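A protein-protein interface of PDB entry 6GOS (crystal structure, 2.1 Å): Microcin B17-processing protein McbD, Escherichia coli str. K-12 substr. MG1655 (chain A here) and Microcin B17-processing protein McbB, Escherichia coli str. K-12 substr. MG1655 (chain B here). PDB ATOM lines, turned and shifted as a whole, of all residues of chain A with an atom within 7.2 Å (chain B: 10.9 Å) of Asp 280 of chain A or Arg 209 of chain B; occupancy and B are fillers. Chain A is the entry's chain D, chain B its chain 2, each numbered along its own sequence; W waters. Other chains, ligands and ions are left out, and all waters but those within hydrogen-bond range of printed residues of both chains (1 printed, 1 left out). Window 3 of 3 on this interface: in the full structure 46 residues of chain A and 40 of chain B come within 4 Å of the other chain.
OD2 of Asp 280 of chain A lies within salt-bridge range of NH2 of Arg 209 of chain B, 3.7 Å away. N of Phe 208 of chain B is in hydrogen-bond range of O of Arg 37 of chain A, at 2.9 Å. The guanidinium group (NE) of Arg 37 of chain A lies within salt-bridge range of the side-chain carboxylate (OE2) of Glu 204 of chain B (3.0 Å). OE2 of Glu 36 of chain A lies within salt-bridge range of NH2 of Arg 209 of chain B, 2.9 Å away. The backbone carbonyl oxygen (O) of Asn 66 of chain A is in hydrogen-bond range of the side-chain hydroxyl (OG) of Ser 202 of chain B. The backbone carbonyl oxygen (O) of Lys 206 of chain B sits at hydrogen-bond distance from the side-chain amide nitrogen (ND2) of Asn 66 of chain A (2.9 Å). The backbone NH (N) of Phe 208 of chain B lies within hydrogen-bond range of the backbone carbonyl oxygen (O) of Glu 36 of chain A (3.4 Å). The guanidinium group (NH2) of Arg 203 of chain B sits close to the guanidinium group (NH1) of Arg 37 of chain A (3.1 Å).
The backbone carbonyl oxygen of Arg 203 of chain B lies within hydrogen-bond range of the side-chain hydroxyl of Ser 207 of chain B (2.6 Å). ND2 of Asn 66 of chain A sits at hydrogen-bond distance from O of Arg 37 of chain A, at 3.0 Å. O of Glu 204 of chain B lies within hydrogen-bond range of OG of Ser 207 of chain B. The side-chain hydroxyl of Ser 214 of chain B sits at hydrogen-bond distance from the side-chain carboxylate of Glu 204 of chain B (2.7 Å). The side-chain hydroxyl of Thr 278 of chain A sits close to the backbone NH of Asp 280 of chain A, 3.2 Å away.
Among the printed residues, merely in contact across the chains: Arg 37 of chain A with Ser 207 of chain B, Asn 66 of chain A with Arg 203 of chain B, Asn 66 of chain A with Ser 207 of chain B, Ile 283 of chain A with Phe 208 of chain B and Ile 283 of chain A with Arg 209 of chain B.
Printed residues of chain B within 4 Å of Arg 37 of chain A: Arg 203 (3.1 Å), Glu 204 (3.0 Å), Ser 207 (3.4 Å) and Phe 208 (2.9 Å). Ile 38 of chain A touches none of the printed residues of chain B. Of the printed residues of chain B, Asn 66 of chain A touches Ser 202, Arg 203, Lys 206 and Ser 207. Of chain B, only Arg 209 comes within 4 Å of Asp 280 of chain A. No residue of chain B comes within 4 Å of Asp 281 of chain A. Ile 283 of chain A touches just these residues of chain B: Phe 208 (3.7 Å) and Arg 209 (3.4 Å). Of the printed residues of chain A, Ser 202 of chain B touches Asn 66 (2.7 Å). Of the printed residues of chain A, Arg 203 of chain B touches Arg 37 (3.1 Å) and Asn 66 (3.4 Å). Of the printed residues of chain A, Lys 206 of chain B touches Asn 66 (2.9 Å). Arg 209 of chain B touches three residues of chain A. The nearest residue of chain B that does not touch Asp 280 of chain A is Arg 210 of chain B (10.0 Å).
Printed residues of chain A that touch a printed residue of chain B: Glu 36, Arg 37, Asn 66, Asp 280 and Ile 283. Of the 14 printed residues of chain B, 7 touch a printed residue of chain A. Hydrophobic or aromatic side chains of chain B within 4 Å of the printed part of chain A: Phe 208. Among the printed residues, 13 pairs touch across the chains. Among the printed residues, Asp or Glu carboxylates within 4 Å of a Lys or Arg side-chain nitrogen of the other chain: Glu 36 of chain A with Arg 209 of chain B, Arg 37 of chain A with Glu 204 of chain B and Asp 280 of chain A with Arg 209 of chain B.
Water W1 lies within hydrogen-bond range of OE2 of Glu 204 of chain B, NE of Arg 203 of chain B and NH2 of Arg 37 of chain A.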
ATOM      1  N   TYR A  35      31.288   8.443  20.285  1.00  0.00           N
ATOM      2  CA  TYR A  35      30.337   7.946  21.278  1.00  0.00           C
ATOM      3  C   TYR A  35      30.028   9.068  22.270  1.00  0.00           C
ATOM      4  O   TYR A  35      29.720  10.172  21.829  1.00  0.00           O
ATOM      5  CB  TYR A  35      30.809   6.619  21.939  1.00  0.00           C
ATOM      6  CG  TYR A  35      31.278   5.592  20.931  1.00  0.00           C
ATOM      7  CD1 TYR A  35      30.381   4.788  20.242  1.00  0.00           C
ATOM      8  CD2 TYR A  35      32.630   5.462  20.640  1.00  0.00           C
ATOM      9  CE1 TYR A  35      30.829   3.876  19.286  1.00  0.00           C
ATOM     10  CE2 TYR A  35      33.082   4.562  19.715  1.00  0.00           C
ATOM     11  CZ  TYR A  35      32.189   3.774  19.035  1.00  0.00           C
ATOM     12  OH  TYR A  35      32.687   2.892  18.117  1.00  0.00           O
ATOM     13  N   GLU A  36      30.099   8.802  23.574  1.00  0.00           N
ATOM     14  CA  GLU A  36      29.952   9.830  24.572  1.00  0.00           C
ATOM     15  C   GLU A  36      31.221   9.913  25.411  1.00  0.00           C
ATOM     16  O   GLU A  36      31.177  10.349  26.585  1.00  0.00           O
ATOM     17  CB  GLU A  36      28.722   9.547  25.425  1.00  0.00           C
ATOM     18  CG  GLU A  36      27.438   9.666  24.632  1.00  0.00           C
ATOM     19  CD  GLU A  36      26.196   9.343  25.444  1.00  0.00           C
ATOM     20  OE1 GLU A  36      26.252   8.532  26.388  1.00  0.00           O
ATOM     21  OE2 GLU A  36      25.137   9.891  25.106  1.00  0.00           O
ATOM     22  N   ARG A  37      32.349   9.531  24.793  1.00  0.00           N
ATOM     23  CA  ARG A  37      33.661   9.713  25.401  1.00  0.00           C
ATOM     24  C   ARG A  37      33.925  11.219  25.595  1.00  0.00           C
ATOM     25  O   ARG A  37      34.408  11.651  26.665  1.00  0.00           O
ATOM     26  CB  ARG A  37      34.763   9.090  24.544  1.00  0.00           C
ATOM     27  CG  ARG A  37      34.743   7.574  24.499  1.00  0.00           C
ATOM     28  CD  ARG A  37      35.319   7.054  23.172  1.00  0.00           C
ATOM     29  NE  ARG A  37      35.519   5.614  23.203  1.00  0.00           N
ATOM     30  CZ  ARG A  37      35.939   4.866  22.174  1.00  0.00           C
ATOM     31  NH1 ARG A  37      36.251   5.416  20.990  1.00  0.00           N
ATOM     32  NH2 ARG A  37      36.075   3.548  22.342  1.00  0.00           N
ATOM     33  N   ILE A  38      33.634  11.975  24.530  1.00  0.00           N
ATOM     34  CA  ILE A  38      33.467  13.440  24.536  1.00  0.00           C
ATOM     35  C   ILE A  38      32.242  13.763  23.704  1.00  0.00           C
ATOM     36  O   ILE A  38      31.706  12.876  23.018  1.00  0.00           O
ATOM     37  CB  ILE A  38      34.680  14.196  23.926  1.00  0.00           C
ATOM     38  CG1 ILE A  38      34.997  13.702  22.491  1.00  0.00           C
ATOM     39  CG2 ILE A  38      35.892  14.043  24.839  1.00  0.00           C
ATOM     40  CD1 ILE A  38      36.111  14.469  21.799  1.00  0.00           C
ATOM     41  N   ASN A  66      39.571  13.241  28.865  1.00  0.00           N
ATOM     42  CA  ASN A  66      39.730  11.769  28.975  1.00  0.00           C
ATOM     43  C   ASN A  66      41.112  11.252  29.325  1.00  0.00           C
ATOM     44  O   ASN A  66      41.226  10.043  29.625  1.00  0.00           O
ATOM     45  CB  ASN A  66      39.385  11.060  27.658  1.00  0.00           C
ATOM     46  CG  ASN A  66      37.997  11.343  27.150  1.00  0.00           C
ATOM     47  OD1 ASN A  66      37.786  11.308  25.930  1.00  0.00           O
ATOM     48  ND2 ASN A  66      37.036  11.588  28.054  1.00  0.00           N
ATOM     49  N   PHE A 272      20.377  19.761  15.477  1.00  0.00           N
ATOM     50  CA  PHE A 272      19.901  19.048  16.654  1.00  0.00           C
ATOM     51  C   PHE A 272      18.362  19.132  16.751  1.00  0.00           C
ATOM     52  O   PHE A 272      17.677  18.118  16.970  1.00  0.00           O
ATOM     53  CB  PHE A 272      20.574  19.614  17.912  1.00  0.00           C
ATOM     54  CG  PHE A 272      20.234  18.872  19.159  1.00  0.00           C
ATOM     55  CD1 PHE A 272      19.088  19.187  19.880  1.00  0.00           C
ATOM     56  CD2 PHE A 272      21.045  17.829  19.604  1.00  0.00           C
ATOM     57  CE1 PHE A 272      18.757  18.482  21.026  1.00  0.00           C
ATOM     58  CE2 PHE A 272      20.713  17.119  20.753  1.00  0.00           C
ATOM     59  CZ  PHE A 272      19.580  17.455  21.459  1.00  0.00           C
ATOM     60  N   TYR A 277      16.201  15.249  18.194  1.00  0.00           N
ATOM     61  CA  TYR A 277      16.983  14.668  19.283  1.00  0.00           C
ATOM     62  C   TYR A 277      16.462  15.150  20.643  1.00  0.00           C
ATOM     63  O   TYR A 277      15.895  16.235  20.751  1.00  0.00           O
ATOM     64  CB  TYR A 277      18.464  15.018  19.130  1.00  0.00           C
ATOM     65  CG  TYR A 277      19.084  14.421  17.889  1.00  0.00           C
ATOM     66  CD1 TYR A 277      19.337  13.053  17.793  1.00  0.00           C
ATOM     67  CD2 TYR A 277      19.389  15.223  16.793  1.00  0.00           C
ATOM     68  CE1 TYR A 277      19.890  12.511  16.640  1.00  0.00           C
ATOM     69  CE2 TYR A 277      19.941  14.699  15.642  1.00  0.00           C
ATOM     70  CZ  TYR A 277      20.195  13.350  15.564  1.00  0.00           C
ATOM     71  OH  TYR A 277      20.748  12.867  14.404  1.00  0.00           O
ATOM     72  N   THR A 278      16.687  14.332  21.667  1.00  0.00           N
ATOM     73  CA  THR A 278      16.076  14.501  22.994  1.00  0.00           C
ATOM     74  C   THR A 278      17.053  15.181  23.939  1.00  0.00           C
ATOM     75  O   THR A 278      18.258  15.224  23.673  1.00  0.00           O
ATOM     76  CB  THR A 278      15.685  13.136  23.595  1.00  0.00           C
ATOM     77  OG1 THR A 278      16.838  12.498  24.166  1.00  0.00           O
ATOM     78  CG2 THR A 278      15.099  12.216  22.523  1.00  0.00           C
ATOM     79  N   ASP A 279      16.524  15.682  25.051  1.00  0.00           N
ATOM     80  CA  ASP A 279      17.339  16.249  26.143  1.00  0.00           C
ATOM     81  C   ASP A 279      18.384  15.270  26.707  1.00  0.00           C
ATOM     82  O   ASP A 279      19.480  15.687  27.107  1.00  0.00           O
ATOM     83  CB  ASP A 279      16.444  16.771  27.290  1.00  0.00           C
ATOM     84  CG  ASP A 279      15.965  18.202  27.065  1.00  0.00           C
ATOM     85  OD1 ASP A 279      16.801  19.078  26.752  1.00  0.00           O
ATOM     86  OD2 ASP A 279      14.754  18.459  27.229  1.00  0.00           O
ATOM     87  N   ASP A 280      18.056  13.978  26.710  1.00  0.00           N
ATOM     88  CA  ASP A 280      18.980  12.951  27.175  1.00  0.00           C
ATOM     89  C   ASP A 280      20.209  12.770  26.272  1.00  0.00           C
ATOM     90  O   ASP A 280      21.194  12.163  26.693  1.00  0.00           O
ATOM     91  CB  ASP A 280      18.257  11.614  27.347  1.00  0.00           C
ATOM     92  CG  ASP A 280      19.043  10.644  28.206  1.00  0.00           C
ATOM     93  OD1 ASP A 280      19.222  10.924  29.417  1.00  0.00           O
ATOM     94  OD2 ASP A 280      19.504   9.621  27.660  1.00  0.00           O
ATOM     95  N   ASP A 281      20.150  13.276  25.038  1.00  0.00           N
ATOM     96  CA  ASP A 281      21.326  13.297  24.157  1.00  0.00           C
ATOM     97  C   ASP A 281      22.325  14.391  24.512  1.00  0.00           C
ATOM     98  O   ASP A 281      23.472  14.317  24.071  1.00  0.00           O
ATOM     99  CB  ASP A 281      20.913  13.466  22.693  1.00  0.00           C
ATOM    100  CG  ASP A 281      20.061  12.318  22.189  1.00  0.00           C
ATOM    101  OD1 ASP A 281      20.293  11.167  22.622  1.00  0.00           O
ATOM    102  OD2 ASP A 281      19.159  12.571  21.358  1.00  0.00           O
ATOM    103  N   ILE A 282      21.879  15.402  25.267  1.00  0.00           N
ATOM    104  CA  ILE A 282      22.735  16.487  25.759  1.00  0.00           C
ATOM    105  C   ILE A 282      23.346  16.065  27.091  1.00  0.00           C
ATOM    106  O   ILE A 282      22.613  15.873  28.071  1.00  0.00           O
ATOM    107  CB  ILE A 282      21.954  17.823  25.943  1.00  0.00           C
ATOM    108  CG1 ILE A 282      21.200  18.222  24.664  1.00  0.00           C
ATOM    109  CG2 ILE A 282      22.900  18.956  26.355  1.00  0.00           C
ATOM    110  CD1 ILE A 282      22.094  18.327  23.434  1.00  0.00           C
ATOM    111  N   ILE A 283      24.671  15.904  27.106  1.00  0.00           N
ATOM    112  CA  ILE A 283      25.445  15.517  28.299  1.00  0.00           C
ATOM    113  C   ILE A 283      26.317  16.643  28.888  1.00  0.00           C
ATOM    114  O   ILE A 283      26.935  16.456  29.946  1.00  0.00           O
ATOM    115  CB  ILE A 283      26.346  14.279  28.018  1.00  0.00           C
ATOM    116  CG1 ILE A 283      27.531  14.604  27.088  1.00  0.00           C
ATOM    117  CG2 ILE A 283      25.505  13.136  27.457  1.00  0.00           C
ATOM    118  CD1 ILE A 283      28.344  13.391  26.671  1.00  0.00           C
ATOM    119  N   ARG A 288      23.634  22.471  27.467  1.00  0.00           N
ATOM    120  CA  ARG A 288      22.270  22.483  27.993  1.00  0.00           C
ATOM    121  C   ARG A 288      21.835  23.925  28.314  1.00  0.00           C
ATOM    122  O   ARG A 288      20.756  24.361  27.915  1.00  0.00           O
ATOM    123  CB  ARG A 288      22.130  21.558  29.224  1.00  0.00           C
ATOM    124  CG  ARG A 288      20.687  21.227  29.591  1.00  0.00           C
ATOM    125  CD  ARG A 288      20.542  20.202  30.723  1.00  0.00           C
ATOM    126  NE  ARG A 288      21.164  18.910  30.394  1.00  0.00           N
ATOM    127  CZ  ARG A 288      22.330  18.451  30.862  1.00  0.00           C
ATOM    128  NH1 ARG A 288      23.069  19.136  31.739  1.00  0.00           N
ATOM    129  NH2 ARG A 288      22.766  17.266  30.454  1.00  0.00           N
ATOM    130  N   SER B 202      41.864   4.457  29.639  1.00  0.00           N
ATOM    131  CA  SER B 202      41.681   5.780  30.240  1.00  0.00           C
ATOM    132  C   SER B 202      40.460   6.483  29.651  1.00  0.00           C
ATOM    133  O   SER B 202      39.605   7.017  30.391  1.00  0.00           O
ATOM    134  CB  SER B 202      42.938   6.635  30.052  1.00  0.00           C
ATOM    135  OG  SER B 202      42.733   7.969  30.491  1.00  0.00           O
ATOM    136  N   ARG B 203      40.358   6.441  28.322  1.00  0.00           N
ATOM    137  CA  ARG B 203      39.282   7.121  27.624  1.00  0.00           C
ATOM    138  C   ARG B 203      37.915   6.538  28.003  1.00  0.00           C
ATOM    139  O   ARG B 203      36.951   7.303  28.139  1.00  0.00           O
ATOM    140  CB  ARG B 203      39.525   7.131  26.111  1.00  0.00           C
ATOM    141  CG  ARG B 203      38.607   8.054  25.287  1.00  0.00           C
ATOM    142  CD  ARG B 203      38.838   7.987  23.756  1.00  0.00           C
ATOM    143  NE  ARG B 203      38.846   6.601  23.257  1.00  0.00           N
ATOM    144  CZ  ARG B 203      39.236   6.217  22.033  1.00  0.00           C
ATOM    145  NH1 ARG B 203      39.601   7.103  21.094  1.00  0.00           N
ATOM    146  NH2 ARG B 203      39.233   4.930  21.729  1.00  0.00           N
ATOM    147  N   GLU B 204      37.834   5.211  28.184  1.00  0.00           N
ATOM    148  CA  GLU B 204      36.611   4.566  28.699  1.00  0.00           C
ATOM    149  C   GLU B 204      36.313   5.003  30.148  1.00  0.00           C
ATOM    150  O   GLU B 204      35.190   5.425  30.428  1.00  0.00           O
ATOM    151  CB  GLU B 204      36.680   3.030  28.620  1.00  0.00           C
ATOM    152  CG  GLU B 204      36.785   2.431  27.223  1.00  0.00           C
ATOM    153  CD  GLU B 204      35.666   2.868  26.299  1.00  0.00           C
ATOM    154  OE1 GLU B 204      34.504   2.470  26.522  1.00  0.00           O
ATOM    155  OE2 GLU B 204      35.958   3.632  25.362  1.00  0.00           O
ATOM    156  N   GLU B 205      37.323   4.936  31.032  1.00  0.00           N
ATOM    157  CA  GLU B 205      37.176   5.292  32.464  1.00  0.00           C
ATOM    158  C   GLU B 205      36.801   6.754  32.657  1.00  0.00           C
ATOM    159  O   GLU B 205      35.948   7.098  33.497  1.00  0.00           O
ATOM    160  CB  GLU B 205      38.480   5.021  33.230  1.00  0.00           C
ATOM    161  N   LYS B 206      37.422   7.619  31.858  1.00  0.00           N
ATOM    162  CA  LYS B 206      37.187   9.052  31.959  1.00  0.00           C
ATOM    163  C   LYS B 206      36.211   9.629  30.902  1.00  0.00           C
ATOM    164  O   LYS B 206      36.168  10.859  30.707  1.00  0.00           O
ATOM    165  CB  LYS B 206      38.531   9.771  31.985  1.00  0.00           C
ATOM    166  CG  LYS B 206      39.380   9.355  33.177  1.00  0.00           C
ATOM    167  CD  LYS B 206      40.711  10.092  33.260  1.00  0.00           C
ATOM    168  CE  LYS B 206      41.381   9.872  34.609  1.00  0.00           C
ATOM    169  NZ  LYS B 206      42.800  10.318  34.589  1.00  0.00           N
ATOM    170  N   SER B 207      35.391   8.772  30.293  1.00  0.00           N
ATOM    171  CA  SER B 207      34.338   9.217  29.370  1.00  0.00           C
ATOM    172  C   SER B 207      33.387  10.237  29.973  1.00  0.00           C
ATOM    173  O   SER B 207      32.948  10.082  31.114  1.00  0.00           O
ATOM    174  CB  SER B 207      33.536   8.031  28.839  1.00  0.00           C
ATOM    175  OG  SER B 207      34.320   7.360  27.881  1.00  0.00           O
ATOM    176  N   PHE B 208      33.098  11.299  29.208  1.00  0.00           N
ATOM    177  CA  PHE B 208      32.182  12.355  29.640  1.00  0.00           C
ATOM    178  C   PHE B 208      30.893  11.731  30.187  1.00  0.00           C
ATOM    179  O   PHE B 208      30.456  12.085  31.270  1.00  0.00           O
ATOM    180  CB  PHE B 208      31.851  13.331  28.484  1.00  0.00           C
ATOM    181  CG  PHE B 208      31.401  14.717  28.922  1.00  0.00           C
ATOM    182  CD1 PHE B 208      31.167  15.069  30.270  1.00  0.00           C
ATOM    183  CD2 PHE B 208      31.184  15.691  27.959  1.00  0.00           C
ATOM    184  CE1 PHE B 208      30.748  16.356  30.618  1.00  0.00           C
ATOM    185  CE2 PHE B 208      30.761  16.973  28.306  1.00  0.00           C
ATOM    186  CZ  PHE B 208      30.538  17.306  29.638  1.00  0.00           C
ATOM    187  N   ARG B 209      30.303  10.810  29.417  1.00  0.00           N
ATOM    188  CA  ARG B 209      29.281   9.876  29.925  1.00  0.00           C
ATOM    189  C   ARG B 209      29.716   8.436  29.677  1.00  0.00           C
ATOM    190  O   ARG B 209      29.729   7.980  28.522  1.00  0.00           O
ATOM    191  CB  ARG B 209      27.900  10.108  29.300  1.00  0.00           C
ATOM    192  CG  ARG B 209      26.825   9.220  29.939  1.00  0.00           C
ATOM    193  CD  ARG B 209      25.440   9.849  29.979  1.00  0.00           C
ATOM    194  NE  ARG B 209      24.774   9.786  28.685  1.00  0.00           N
ATOM    195  CZ  ARG B 209      23.636  10.414  28.381  1.00  0.00           C
ATOM    196  NH1 ARG B 209      23.001  11.170  29.284  1.00  0.00           N
ATOM    197  NH2 ARG B 209      23.115  10.285  27.154  1.00  0.00           N
ATOM    198  N   ARG B 210      30.088   7.733  30.752  1.00  0.00           N
ATOM    199  CA  ARG B 210      30.588   6.354  30.646  1.00  0.00           C
ATOM    200  C   ARG B 210      29.486   5.514  30.032  1.00  0.00           C
ATOM    201  O   ARG B 210      28.307   5.630  30.402  1.00  0.00           O
ATOM    202  CB  ARG B 210      30.982   5.738  32.019  1.00  0.00           C
ATOM    203  CG  ARG B 210      32.262   6.263  32.692  1.00  0.00           C
ATOM    204  CD  ARG B 210      32.655   5.429  33.927  1.00  0.00           C
ATOM    205  N   ASN B 211      29.885   4.720  29.051  1.00  0.00           N
ATOM    206  CA  ASN B 211      29.098   3.620  28.547  1.00  0.00           C
ATOM    207  C   ASN B 211      29.164   2.493  29.599  1.00  0.00           C
ATOM    208  O   ASN B 211      30.217   1.867  29.771  1.00  0.00           O
ATOM    209  CB  ASN B 211      29.691   3.158  27.201  1.00  0.00           C
ATOM    210  CG  ASN B 211      28.992   1.936  26.631  1.00  0.00           C
ATOM    211  OD1 ASN B 211      27.899   1.570  27.056  1.00  0.00           O
ATOM    212  ND2 ASN B 211      29.627   1.296  25.667  1.00  0.00           N
ATOM    213  N   GLU B 212      28.050   2.226  30.286  1.00  0.00           N
ATOM    214  CA  GLU B 212      28.005   1.146  31.294  1.00  0.00           C
ATOM    215  C   GLU B 212      28.303  -0.263  30.719  1.00  0.00           C
ATOM    216  O   GLU B 212      28.690  -1.156  31.459  1.00  0.00           O
ATOM    217  CB  GLU B 212      26.669   1.157  32.041  1.00  0.00           C
ATOM    218  N   MET B 213      28.162  -0.430  29.398  1.00  0.00           N
ATOM    219  CA  MET B 213      28.506  -1.656  28.680  1.00  0.00           C
ATOM    220  C   MET B 213      29.822  -1.547  27.898  1.00  0.00           C
ATOM    221  O   MET B 213      29.980  -2.198  26.868  1.00  0.00           O
ATOM    222  CB  MET B 213      27.370  -1.982  27.710  1.00  0.00           C
ATOM    223  CG  MET B 213      26.024  -2.235  28.372  1.00  0.00           C
ATOM    224  SD  MET B 213      26.068  -3.706  29.427  1.00  0.00           S
ATOM    225  CE  MET B 213      26.094  -3.013  31.090  1.00  0.00           C
ATOM    226  N   SER B 214      30.748  -0.709  28.362  1.00  0.00           N
ATOM    227  CA  SER B 214      32.100  -0.625  27.778  1.00  0.00           C
ATOM    228  C   SER B 214      32.837  -1.976  27.845  1.00  0.00           C
ATOM    229  O   SER B 214      32.734  -2.694  28.844  1.00  0.00           O
ATOM    230  CB  SER B 214      32.942   0.445  28.501  1.00  0.00           C
ATOM    231  OG  SER B 214      34.314   0.355  28.144  1.00  0.00           O
ATOM    232  N   ASN B 217      34.956  -2.711  30.923  1.00  0.00           N
ATOM    233  CA  ASN B 217      34.428  -3.457  32.065  1.00  0.00           C
ATOM    234  C   ASN B 217      34.910  -4.900  32.064  1.00  0.00           C
ATOM    235  O   ASN B 217      35.260  -5.432  33.116  1.00  0.00           O
ATOM    236  CB  ASN B 217      32.907  -3.483  32.071  1.00  0.00           C
ATOM    237  CG  ASN B 217      32.296  -2.137  32.337  1.00  0.00           C
ATOM    238  OD1 ASN B 217      32.949  -1.226  32.843  1.00  0.00           O
ATOM    239  ND2 ASN B 217      31.019  -2.002  32.002  1.00  0.00           N
HETATM  240  O   HOH W   1      38.526   4.109  24.608  1.00  0.00           O
